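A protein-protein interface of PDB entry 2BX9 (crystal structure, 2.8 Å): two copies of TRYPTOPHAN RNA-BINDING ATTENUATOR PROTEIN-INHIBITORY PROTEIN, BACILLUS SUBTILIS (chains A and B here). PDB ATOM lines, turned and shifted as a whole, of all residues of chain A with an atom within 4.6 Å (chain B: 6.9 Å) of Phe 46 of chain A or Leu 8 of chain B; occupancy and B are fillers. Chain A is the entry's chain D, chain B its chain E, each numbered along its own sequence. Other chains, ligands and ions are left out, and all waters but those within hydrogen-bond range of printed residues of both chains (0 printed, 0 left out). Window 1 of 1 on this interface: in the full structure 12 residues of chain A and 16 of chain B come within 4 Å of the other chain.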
ATOM      1  N   THR A  42     -28.251 -16.867 -24.648  1.00  0.00           N
ATOM      2  CA  THR A  42     -28.494 -17.293 -23.281  1.00  0.00           C
ATOM      3  C   THR A  42     -28.239 -16.163 -22.295  1.00  0.00           C
ATOM      4  O   THR A  42     -29.117 -15.850 -21.472  1.00  0.00           O
ATOM      5  CB  THR A  42     -27.630 -18.490 -22.960  1.00  0.00           C
ATOM      6  OG1 THR A  42     -28.093 -19.600 -23.728  1.00  0.00           O
ATOM      7  CG2 THR A  42     -27.822 -18.936 -21.520  1.00  0.00           C
ATOM      8  N   LEU A  43     -27.062 -15.549 -22.400  1.00  0.00           N
ATOM      9  CA  LEU A  43     -26.675 -14.439 -21.542  1.00  0.00           C
ATOM     10  C   LEU A  43     -27.570 -13.224 -21.705  1.00  0.00           C
ATOM     11  O   LEU A  43     -27.967 -12.609 -20.718  1.00  0.00           O
ATOM     12  CB  LEU A  43     -25.240 -14.044 -21.823  1.00  0.00           C
ATOM     13  CG  LEU A  43     -24.267 -14.234 -20.667  1.00  0.00           C
ATOM     14  CD1 LEU A  43     -22.995 -14.960 -21.107  1.00  0.00           C
ATOM     15  CD2 LEU A  43     -23.952 -12.856 -20.026  1.00  0.00           C
ATOM     16  N   LEU A  44     -27.891 -12.889 -22.949  1.00  0.00           N
ATOM     17  CA  LEU A  44     -28.644 -11.684 -23.246  1.00  0.00           C
ATOM     18  C   LEU A  44     -30.086 -11.860 -22.785  1.00  0.00           C
ATOM     19  O   LEU A  44     -30.679 -10.936 -22.219  1.00  0.00           O
ATOM     20  CB  LEU A  44     -28.594 -11.383 -24.741  1.00  0.00           C
ATOM     21  CG  LEU A  44     -28.696  -9.976 -25.345  1.00  0.00           C
ATOM     22  CD1 LEU A  44     -29.321 -10.084 -26.720  1.00  0.00           C
ATOM     23  CD2 LEU A  44     -29.487  -8.974 -24.524  1.00  0.00           C
ATOM     24  N   ASP A  45     -30.649 -13.043 -23.019  1.00  0.00           N
ATOM     25  CA  ASP A  45     -31.999 -13.316 -22.565  1.00  0.00           C
ATOM     26  C   ASP A  45     -32.158 -13.223 -21.051  1.00  0.00           C
ATOM     27  O   ASP A  45     -33.092 -12.586 -20.562  1.00  0.00           O
ATOM     28  CB  ASP A  45     -32.460 -14.667 -23.063  1.00  0.00           C
ATOM     29  CG  ASP A  45     -33.090 -14.582 -24.415  1.00  0.00           C
ATOM     30  OD1 ASP A  45     -32.371 -14.819 -25.409  1.00  0.00           O
ATOM     31  OD2 ASP A  45     -34.287 -14.251 -24.581  1.00  0.00           O
ATOM     32  N   PHE A  46     -31.241 -13.850 -20.323  1.00  0.00           N
ATOM     33  CA  PHE A  46     -31.219 -13.765 -18.877  1.00  0.00           C
ATOM     34  C   PHE A  46     -31.210 -12.297 -18.398  1.00  0.00           C
ATOM     35  O   PHE A  46     -32.092 -11.893 -17.625  1.00  0.00           O
ATOM     36  CB  PHE A  46     -30.024 -14.564 -18.340  1.00  0.00           C
ATOM     37  CG  PHE A  46     -29.869 -14.499 -16.855  1.00  0.00           C
ATOM     38  CD1 PHE A  46     -30.701 -15.239 -16.025  1.00  0.00           C
ATOM     39  CD2 PHE A  46     -28.893 -13.694 -16.288  1.00  0.00           C
ATOM     40  CE1 PHE A  46     -30.563 -15.178 -14.656  1.00  0.00           C
ATOM     41  CE2 PHE A  46     -28.739 -13.635 -14.921  1.00  0.00           C
ATOM     42  CZ  PHE A  46     -29.578 -14.373 -14.097  1.00  0.00           C
ATOM     43  N   ILE A  47     -30.247 -11.503 -18.885  1.00  0.00           N
ATOM     44  CA  ILE A  47     -30.122 -10.091 -18.486  1.00  0.00           C
ATOM     45  C   ILE A  47     -31.391  -9.321 -18.802  1.00  0.00           C
ATOM     46  O   ILE A  47     -31.916  -8.620 -17.943  1.00  0.00           O
ATOM     47  CB  ILE A  47     -28.886  -9.372 -19.127  1.00  0.00           C
ATOM     48  CG1 ILE A  47     -27.568 -10.072 -18.763  1.00  0.00           C
ATOM     49  CG2 ILE A  47     -28.840  -7.884 -18.708  1.00  0.00           C
ATOM     50  CD1 ILE A  47     -27.310 -10.235 -17.280  1.00  0.00           C
ATOM     51  N   GLN A  48     -31.887  -9.466 -20.027  1.00  0.00           N
ATOM     52  CA  GLN A  48     -33.122  -8.810 -20.434  1.00  0.00           C
ATOM     53  C   GLN A  48     -34.306  -9.107 -19.528  1.00  0.00           C
ATOM     54  O   GLN A  48     -35.069  -8.199 -19.182  1.00  0.00           O
ATOM     55  CB  GLN A  48     -33.469  -9.154 -21.875  1.00  0.00           C
ATOM     56  CG  GLN A  48     -32.881  -8.171 -22.867  1.00  0.00           C
ATOM     57  CD  GLN A  48     -33.032  -8.589 -24.330  1.00  0.00           C
ATOM     58  OE1 GLN A  48     -32.867  -7.763 -25.228  1.00  0.00           O
ATOM     59  NE2 GLN A  48     -33.332  -9.862 -24.570  1.00  0.00           N
ATOM     60  N   LYS A  49     -34.464 -10.363 -19.126  1.00  0.00           N
ATOM     61  CA  LYS A  49     -35.629 -10.697 -18.332  1.00  0.00           C
ATOM     62  C   LYS A  49     -35.473 -10.386 -16.845  1.00  0.00           C
ATOM     63  O   LYS A  49     -36.469 -10.309 -16.137  1.00  0.00           O
ATOM     64  CB  LYS A  49     -36.137 -12.122 -18.609  1.00  0.00           C
ATOM     65  CG  LYS A  49     -35.480 -13.221 -17.803  1.00  0.00           C
ATOM     66  CD  LYS A  49     -36.181 -14.543 -17.997  1.00  0.00           C
ATOM     67  CE  LYS A  49     -37.381 -14.675 -17.061  1.00  0.00           C
ATOM     68  NZ  LYS A  49     -38.104 -15.965 -17.248  1.00  0.00           N
ATOM     69  N   HIS A  50     -34.251 -10.164 -16.376  1.00  0.00           N
ATOM     70  CA  HIS A  50     -34.062  -9.954 -14.946  1.00  0.00           C
ATOM     71  C   HIS A  50     -33.595  -8.553 -14.573  1.00  0.00           C
ATOM     72  O   HIS A  50     -33.756  -8.115 -13.426  1.00  0.00           O
ATOM     73  CB  HIS A  50     -33.128 -11.017 -14.378  1.00  0.00           C
ATOM     74  CG  HIS A  50     -33.737 -12.379 -14.334  1.00  0.00           C
ATOM     75  ND1 HIS A  50     -34.624 -12.763 -13.352  1.00  0.00           N
ATOM     76  CD2 HIS A  50     -33.588 -13.448 -15.151  1.00  0.00           C
ATOM     77  CE1 HIS A  50     -34.993 -14.012 -13.564  1.00  0.00           C
ATOM     78  NE2 HIS A  50     -34.378 -14.452 -14.650  1.00  0.00           N
ATOM     79  N   ILE B   3     -21.921 -21.840 -19.813  1.00  0.00           N
ATOM     80  CA  ILE B   3     -22.983 -21.450 -18.860  1.00  0.00           C
ATOM     81  C   ILE B   3     -24.369 -21.369 -19.530  1.00  0.00           C
ATOM     82  O   ILE B   3     -24.607 -20.522 -20.390  1.00  0.00           O
ATOM     83  CB  ILE B   3     -22.601 -20.157 -18.040  1.00  0.00           C
ATOM     84  CG1 ILE B   3     -23.757 -19.169 -17.973  1.00  0.00           C
ATOM     85  CG2 ILE B   3     -21.401 -19.431 -18.612  1.00  0.00           C
ATOM     86  CD1 ILE B   3     -23.298 -17.732 -17.736  1.00  0.00           C
ATOM     87  N   ALA B   4     -25.262 -22.284 -19.169  1.00  0.00           N
ATOM     88  CA  ALA B   4     -26.584 -22.318 -19.779  1.00  0.00           C
ATOM     89  C   ALA B   4     -27.607 -21.627 -18.893  1.00  0.00           C
ATOM     90  O   ALA B   4     -27.273 -21.115 -17.829  1.00  0.00           O
ATOM     91  CB  ALA B   4     -27.002 -23.732 -20.072  1.00  0.00           C
ATOM     92  N   THR B   5     -28.857 -21.603 -19.338  1.00  0.00           N
ATOM     93  CA  THR B   5     -29.933 -20.979 -18.571  1.00  0.00           C
ATOM     94  C   THR B   5     -30.108 -21.650 -17.210  1.00  0.00           C
ATOM     95  O   THR B   5     -30.291 -20.985 -16.176  1.00  0.00           O
ATOM     96  CB  THR B   5     -31.244 -21.017 -19.380  1.00  0.00           C
ATOM     97  OG1 THR B   5     -31.009 -20.444 -20.677  1.00  0.00           O
ATOM     98  CG2 THR B   5     -32.282 -20.104 -18.754  1.00  0.00           C
ATOM     99  N   ASP B   6     -30.020 -22.973 -17.224  1.00  0.00           N
ATOM    100  CA  ASP B   6     -30.187 -23.780 -16.028  1.00  0.00           C
ATOM    101  C   ASP B   6     -29.108 -23.577 -14.967  1.00  0.00           C
ATOM    102  O   ASP B   6     -29.309 -23.972 -13.802  1.00  0.00           O
ATOM    103  CB  ASP B   6     -30.317 -25.255 -16.406  1.00  0.00           C
ATOM    104  CG  ASP B   6     -31.756 -25.653 -16.681  1.00  0.00           C
ATOM    105  OD1 ASP B   6     -32.667 -24.841 -16.360  1.00  0.00           O
ATOM    106  OD2 ASP B   6     -32.075 -26.754 -17.195  1.00  0.00           O
ATOM    107  N   ASP B   7     -27.985 -22.969 -15.375  1.00  0.00           N
ATOM    108  CA  ASP B   7     -26.897 -22.568 -14.474  1.00  0.00           C
ATOM    109  C   ASP B   7     -27.177 -21.228 -13.838  1.00  0.00           C
ATOM    110  O   ASP B   7     -26.544 -20.870 -12.841  1.00  0.00           O
ATOM    111  CB  ASP B   7     -25.594 -22.421 -15.243  1.00  0.00           C
ATOM    112  CG  ASP B   7     -25.084 -23.735 -15.800  1.00  0.00           C
ATOM    113  OD1 ASP B   7     -25.689 -24.794 -15.494  1.00  0.00           O
ATOM    114  OD2 ASP B   7     -24.076 -23.793 -16.555  1.00  0.00           O
ATOM    115  N   LEU B   8     -28.117 -20.490 -14.441  1.00  0.00           N
ATOM    116  CA  LEU B   8     -28.453 -19.115 -14.051  1.00  0.00           C
ATOM    117  C   LEU B   8     -29.794 -19.005 -13.295  1.00  0.00           C
ATOM    118  O   LEU B   8     -29.929 -18.189 -12.391  1.00  0.00           O
ATOM    119  CB  LEU B   8     -28.440 -18.200 -15.289  1.00  0.00           C
ATOM    120  CG  LEU B   8     -27.201 -18.154 -16.208  1.00  0.00           C
ATOM    121  CD1 LEU B   8     -27.487 -17.321 -17.455  1.00  0.00           C
ATOM    122  CD2 LEU B   8     -25.980 -17.623 -15.484  1.00  0.00           C
ATOM    123  N   GLU B   9     -30.776 -19.829 -13.663  1.00  0.00           N
ATOM    124  CA  GLU B   9     -32.106 -19.767 -13.046  1.00  0.00           C
ATOM    125  C   GLU B   9     -32.580 -21.157 -12.695  1.00  0.00           C
ATOM    126  O   GLU B   9     -32.307 -22.107 -13.430  1.00  0.00           O
ATOM    127  CB  GLU B   9     -33.168 -19.196 -13.990  1.00  0.00           C
ATOM    128  CG  GLU B   9     -32.781 -18.048 -14.883  1.00  0.00           C
ATOM    129  CD  GLU B   9     -33.881 -17.741 -15.877  1.00  0.00           C
ATOM    130  OE1 GLU B   9     -34.588 -18.689 -16.293  1.00  0.00           O
ATOM    131  OE2 GLU B   9     -34.062 -16.554 -16.229  1.00  0.00           O
ATOM    132  N   VAL B  10     -33.326 -21.256 -11.595  1.00  0.00           N
ATOM    133  CA  VAL B  10     -34.042 -22.466 -11.229  1.00  0.00           C
ATOM    134  C   VAL B  10     -35.552 -22.228 -11.411  1.00  0.00           C
ATOM    135  O   VAL B  10     -36.039 -21.116 -11.213  1.00  0.00           O
ATOM    136  CB  VAL B  10     -33.752 -22.858  -9.770  1.00  0.00           C
ATOM    137  CG1 VAL B  10     -34.481 -24.124  -9.400  1.00  0.00           C
ATOM    138  CG2 VAL B  10     -32.278 -23.078  -9.569  1.00  0.00           C
ATOM    139  N   VAL B  34     -39.304 -17.984 -11.660  1.00  0.00           N
ATOM    140  CA  VAL B  34     -37.931 -18.464 -11.685  1.00  0.00           C
ATOM    141  C   VAL B  34     -37.132 -17.854 -10.507  1.00  0.00           C
ATOM    142  O   VAL B  34     -37.438 -16.754 -10.034  1.00  0.00           O
ATOM    143  CB  VAL B  34     -37.314 -18.170 -13.106  1.00  0.00           C
ATOM    144  CG1 VAL B  34     -36.263 -17.078 -13.074  1.00  0.00           C
ATOM    145  CG2 VAL B  34     -36.765 -19.427 -13.729  1.00  0.00           C
ATOM    146  N   ILE B  35     -36.143 -18.584 -10.007  1.00  0.00           N
ATOM    147  CA  ILE B  35     -35.284 -18.088  -8.924  1.00  0.00           C
ATOM    148  C   ILE B  35     -33.819 -18.125  -9.371  1.00  0.00           C
ATOM    149  O   ILE B  35     -33.384 -19.104  -9.982  1.00  0.00           O
ATOM    150  CB  ILE B  35     -35.480 -18.934  -7.646  1.00  0.00           C
ATOM    151  CG1 ILE B  35     -36.843 -18.658  -7.026  1.00  0.00           C
ATOM    152  CG2 ILE B  35     -34.381 -18.643  -6.630  1.00  0.00           C
ATOM    153  CD1 ILE B  35     -37.345 -19.752  -6.106  1.00  0.00           C
ATOM    154  N   LEU B  36     -33.061 -17.073  -9.066  1.00  0.00           N
ATOM    155  CA  LEU B  36     -31.675 -16.993  -9.520  1.00  0.00           C
ATOM    156  C   LEU B  36     -30.717 -17.805  -8.670  1.00  0.00           C
ATOM    157  O   LEU B  36     -30.923 -17.995  -7.480  1.00  0.00           O
ATOM    158  CB  LEU B  36     -31.190 -15.547  -9.644  1.00  0.00           C
ATOM    159  CG  LEU B  36     -31.896 -14.619 -10.646  1.00  0.00           C
ATOM    160  CD1 LEU B  36     -30.984 -13.495 -11.038  1.00  0.00           C
ATOM    161  CD2 LEU B  36     -32.333 -15.315 -11.888  1.00  0.00           C
ATOM    162  N   THR B  37     -29.675 -18.302  -9.315  1.00  0.00           N
ATOM    163  CA  THR B  37     -28.621 -19.075  -8.669  1.00  0.00           C
ATOM    164  C   THR B  37     -27.482 -18.134  -8.262  1.00  0.00           C
ATOM    165  O   THR B  37     -27.485 -16.953  -8.634  1.00  0.00           O
ATOM    166  CB  THR B  37     -28.069 -20.105  -9.665  1.00  0.00           C
ATOM    167  OG1 THR B  37     -27.698 -19.431 -10.878  1.00  0.00           O
ATOM    168  CG2 THR B  37     -29.148 -21.085 -10.112  1.00  0.00           C
ATOM    169  N   ALA B  38     -26.503 -18.647  -7.520  1.00  0.00           N
ATOM    170  CA  ALA B  38     -25.344 -17.833  -7.162  1.00  0.00           C
ATOM    171  C   ALA B  38     -24.760 -17.239  -8.424  1.00  0.00           C
ATOM    172  O   ALA B  38     -24.416 -16.056  -8.478  1.00  0.00           O
ATOM    173  CB  ALA B  38     -24.308 -18.649  -6.461  1.00  0.00           C
ATOM    174  N   GLN B  39     -24.668 -18.072  -9.453  1.00  0.00           N
ATOM    175  CA  GLN B  39     -24.023 -17.680 -10.691  1.00  0.00           C
ATOM    176  C   GLN B  39     -24.822 -16.613 -11.415  1.00  0.00           C
ATOM    177  O   GLN B  39     -24.242 -15.722 -12.037  1.00  0.00           O
ATOM    178  CB  GLN B  39     -23.803 -18.898 -11.593  1.00  0.00           C
ATOM    179  CG  GLN B  39     -23.324 -18.595 -13.011  1.00  0.00           C
ATOM    180  CD  GLN B  39     -21.844 -18.249 -13.086  1.00  0.00           C
ATOM    181  OE1 GLN B  39     -21.025 -19.109 -13.399  1.00  0.00           O
ATOM    182  NE2 GLN B  39     -21.504 -16.988 -12.811  1.00  0.00           N
ATOM    183  N   GLY B  40     -26.148 -16.710 -11.341  1.00  0.00           N
ATOM    184  CA  GLY B  40     -27.017 -15.803 -12.077  1.00  0.00           C
ATOM    185  C   GLY B  40     -27.055 -14.467 -11.386  1.00  0.00           C
ATOM    186  O   GLY B  40     -27.153 -13.437 -12.036  1.00  0.00           O
ATOM    187  N   TYR B  41     -26.985 -14.494 -10.059  1.00  0.00           N
ATOM    188  CA  TYR B  41     -26.950 -13.277  -9.261  1.00  0.00           C
ATOM    189  C   TYR B  41     -25.632 -12.524  -9.486  1.00  0.00           C
ATOM    190  O   TYR B  41     -25.626 -11.301  -9.615  1.00  0.00           O
ATOM    191  CB  TYR B  41     -27.160 -13.585  -7.771  1.00  0.00           C
ATOM    192  CG  TYR B  41     -27.331 -12.332  -6.953  1.00  0.00           C
ATOM    193  CD1 TYR B  41     -28.510 -11.575  -7.051  1.00  0.00           C
ATOM    194  CD2 TYR B  41     -26.315 -11.880  -6.090  1.00  0.00           C
ATOM    195  CE1 TYR B  41     -28.679 -10.408  -6.301  1.00  0.00           C
ATOM    196  CE2 TYR B  41     -26.477 -10.716  -5.335  1.00  0.00           C
ATOM    197  CZ  TYR B  41     -27.662  -9.992  -5.458  1.00  0.00           C
ATOM    198  OH  TYR B  41     -27.839  -8.840  -4.756  1.00  0.00           O
ATOM    199  N   THR B  42     -24.530 -13.270  -9.546  1.00  0.00           N
ATOM    200  CA  THR B  42     -23.219 -12.719  -9.835  1.00  0.00           C
ATOM    201  C   THR B  42     -23.175 -11.929 -11.151  1.00  0.00           C
ATOM    202  O   THR B  42     -22.743 -10.766 -11.164  1.00  0.00           O
ATOM    203  CB  THR B  42     -22.189 -13.854  -9.860  1.00  0.00           C
ATOM    204  OG1 THR B  42     -21.963 -14.294  -8.525  1.00  0.00           O
ATOM    205  CG2 THR B  42     -20.807 -13.343 -10.290  1.00  0.00           C
ATOM    206  N   LEU B  43     -23.590 -12.571 -12.246  1.00  0.00           N
ATOM    207  CA  LEU B  43     -23.682 -11.918 -13.546  1.00  0.00           C
ATOM    208  C   LEU B  43     -24.546 -10.654 -13.506  1.00  0.00           C
ATOM    209  O   LEU B  43     -24.160  -9.619 -14.024  1.00  0.00           O
ATOM    210  CB  LEU B  43     -24.282 -12.863 -14.588  1.00  0.00           C
ATOM    211  CG  LEU B  43     -23.534 -14.066 -15.179  1.00  0.00           C
ATOM    212  CD1 LEU B  43     -24.195 -14.416 -16.525  1.00  0.00           C
ATOM    213  CD2 LEU B  43     -22.003 -13.871 -15.361  1.00  0.00           C
ATOM    214  N   LEU B  44     -25.720 -10.759 -12.886  1.00  0.00           N
ATOM    215  CA  LEU B  44     -26.741  -9.717 -12.942  1.00  0.00           C
ATOM    216  C   LEU B  44     -26.350  -8.523 -12.086  1.00  0.00           C
ATOM    217  O   LEU B  44     -26.653  -7.378 -12.442  1.00  0.00           O
ATOM    218  CB  LEU B  44     -28.123 -10.282 -12.560  1.00  0.00           C
ATOM    219  CG  LEU B  44     -29.313  -9.322 -12.388  1.00  0.00           C
ATOM    220  CD1 LEU B  44     -29.613  -8.533 -13.641  1.00  0.00           C
ATOM    221  CD2 LEU B  44     -30.559 -10.046 -11.953  1.00  0.00           C
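Leu 43 of chain B touches its own counterpart, Leu 43 of chain A. Positions printed for both chains: 42, 43 and 44.
Along chain A the printed residues that touch a printed residue of chain B span positions 42 to 50. Among the printed residues, 13 pairs touch across the chains.
N of Ala 4 of chain B is in hydrogen-bond range of OD2 of Asp 7 of chain B (3.2 Å). O of Leu 8 of chain B is in hydrogen-bond range of OG1 of Thr 37 of chain B (3.0 Å). N of Gly 40 of chain B sits at hydrogen-bond distance from OG1 of Thr 37 of chain B, at 3.2 Å.
A ring nitrogen (NE2) of His 50 of chain A lies within hydrogen-bond range of the side-chain carboxylate (OE2) of Glu 9 of chain B (2.6 Å).
Among the printed residues, pairs that only touch across the chains: Phe 46 of chain A with Leu 36 of chain B, Phe 46 of chain A with Gly 40 of chain B, His 50 of chain A with Val 34 of chain B, His 50 of chain A with Leu 36 of chain B, Lys 49 of chain A with Glu 9 of chain B, Thr 42 of chain A with Thr 5 of chain B, Phe 46 of chain A with Glu 9 of chain B, His 50 of chain A with Leu 44 of chain B, Phe 46 of chain A with Leu 8 of chain B, Thr 42 of chain A with Ile 3 of chain B, Thr 42 of chain A with Ala 4 of chain B and Leu 43 of chain A with Leu 43 of chain B.
Of the printed residues of chain B, Leu 43 of chain A touches Leu 43. Of the printed residues of chain B, Phe 46 of chain A touches Leu 8, Glu 9, Leu 36 and Gly 40. Printed residues of chain A within 4 Å of Ala 4 of chain B: Thr 42. Leu 8 of chain B touches just one residue of chain A: Phe 46 (3.7 Å). Thr 42 of chain B touches none of the printed residues of chain A. The nearest residue of chain A that does not touch Leu 8 of chain B is Thr 42 of chain A (4.4 Å). The nearest printed residue of chain A that does not touch Leu 43 of chain B is Phe 46 of chain A (4.5 Å).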
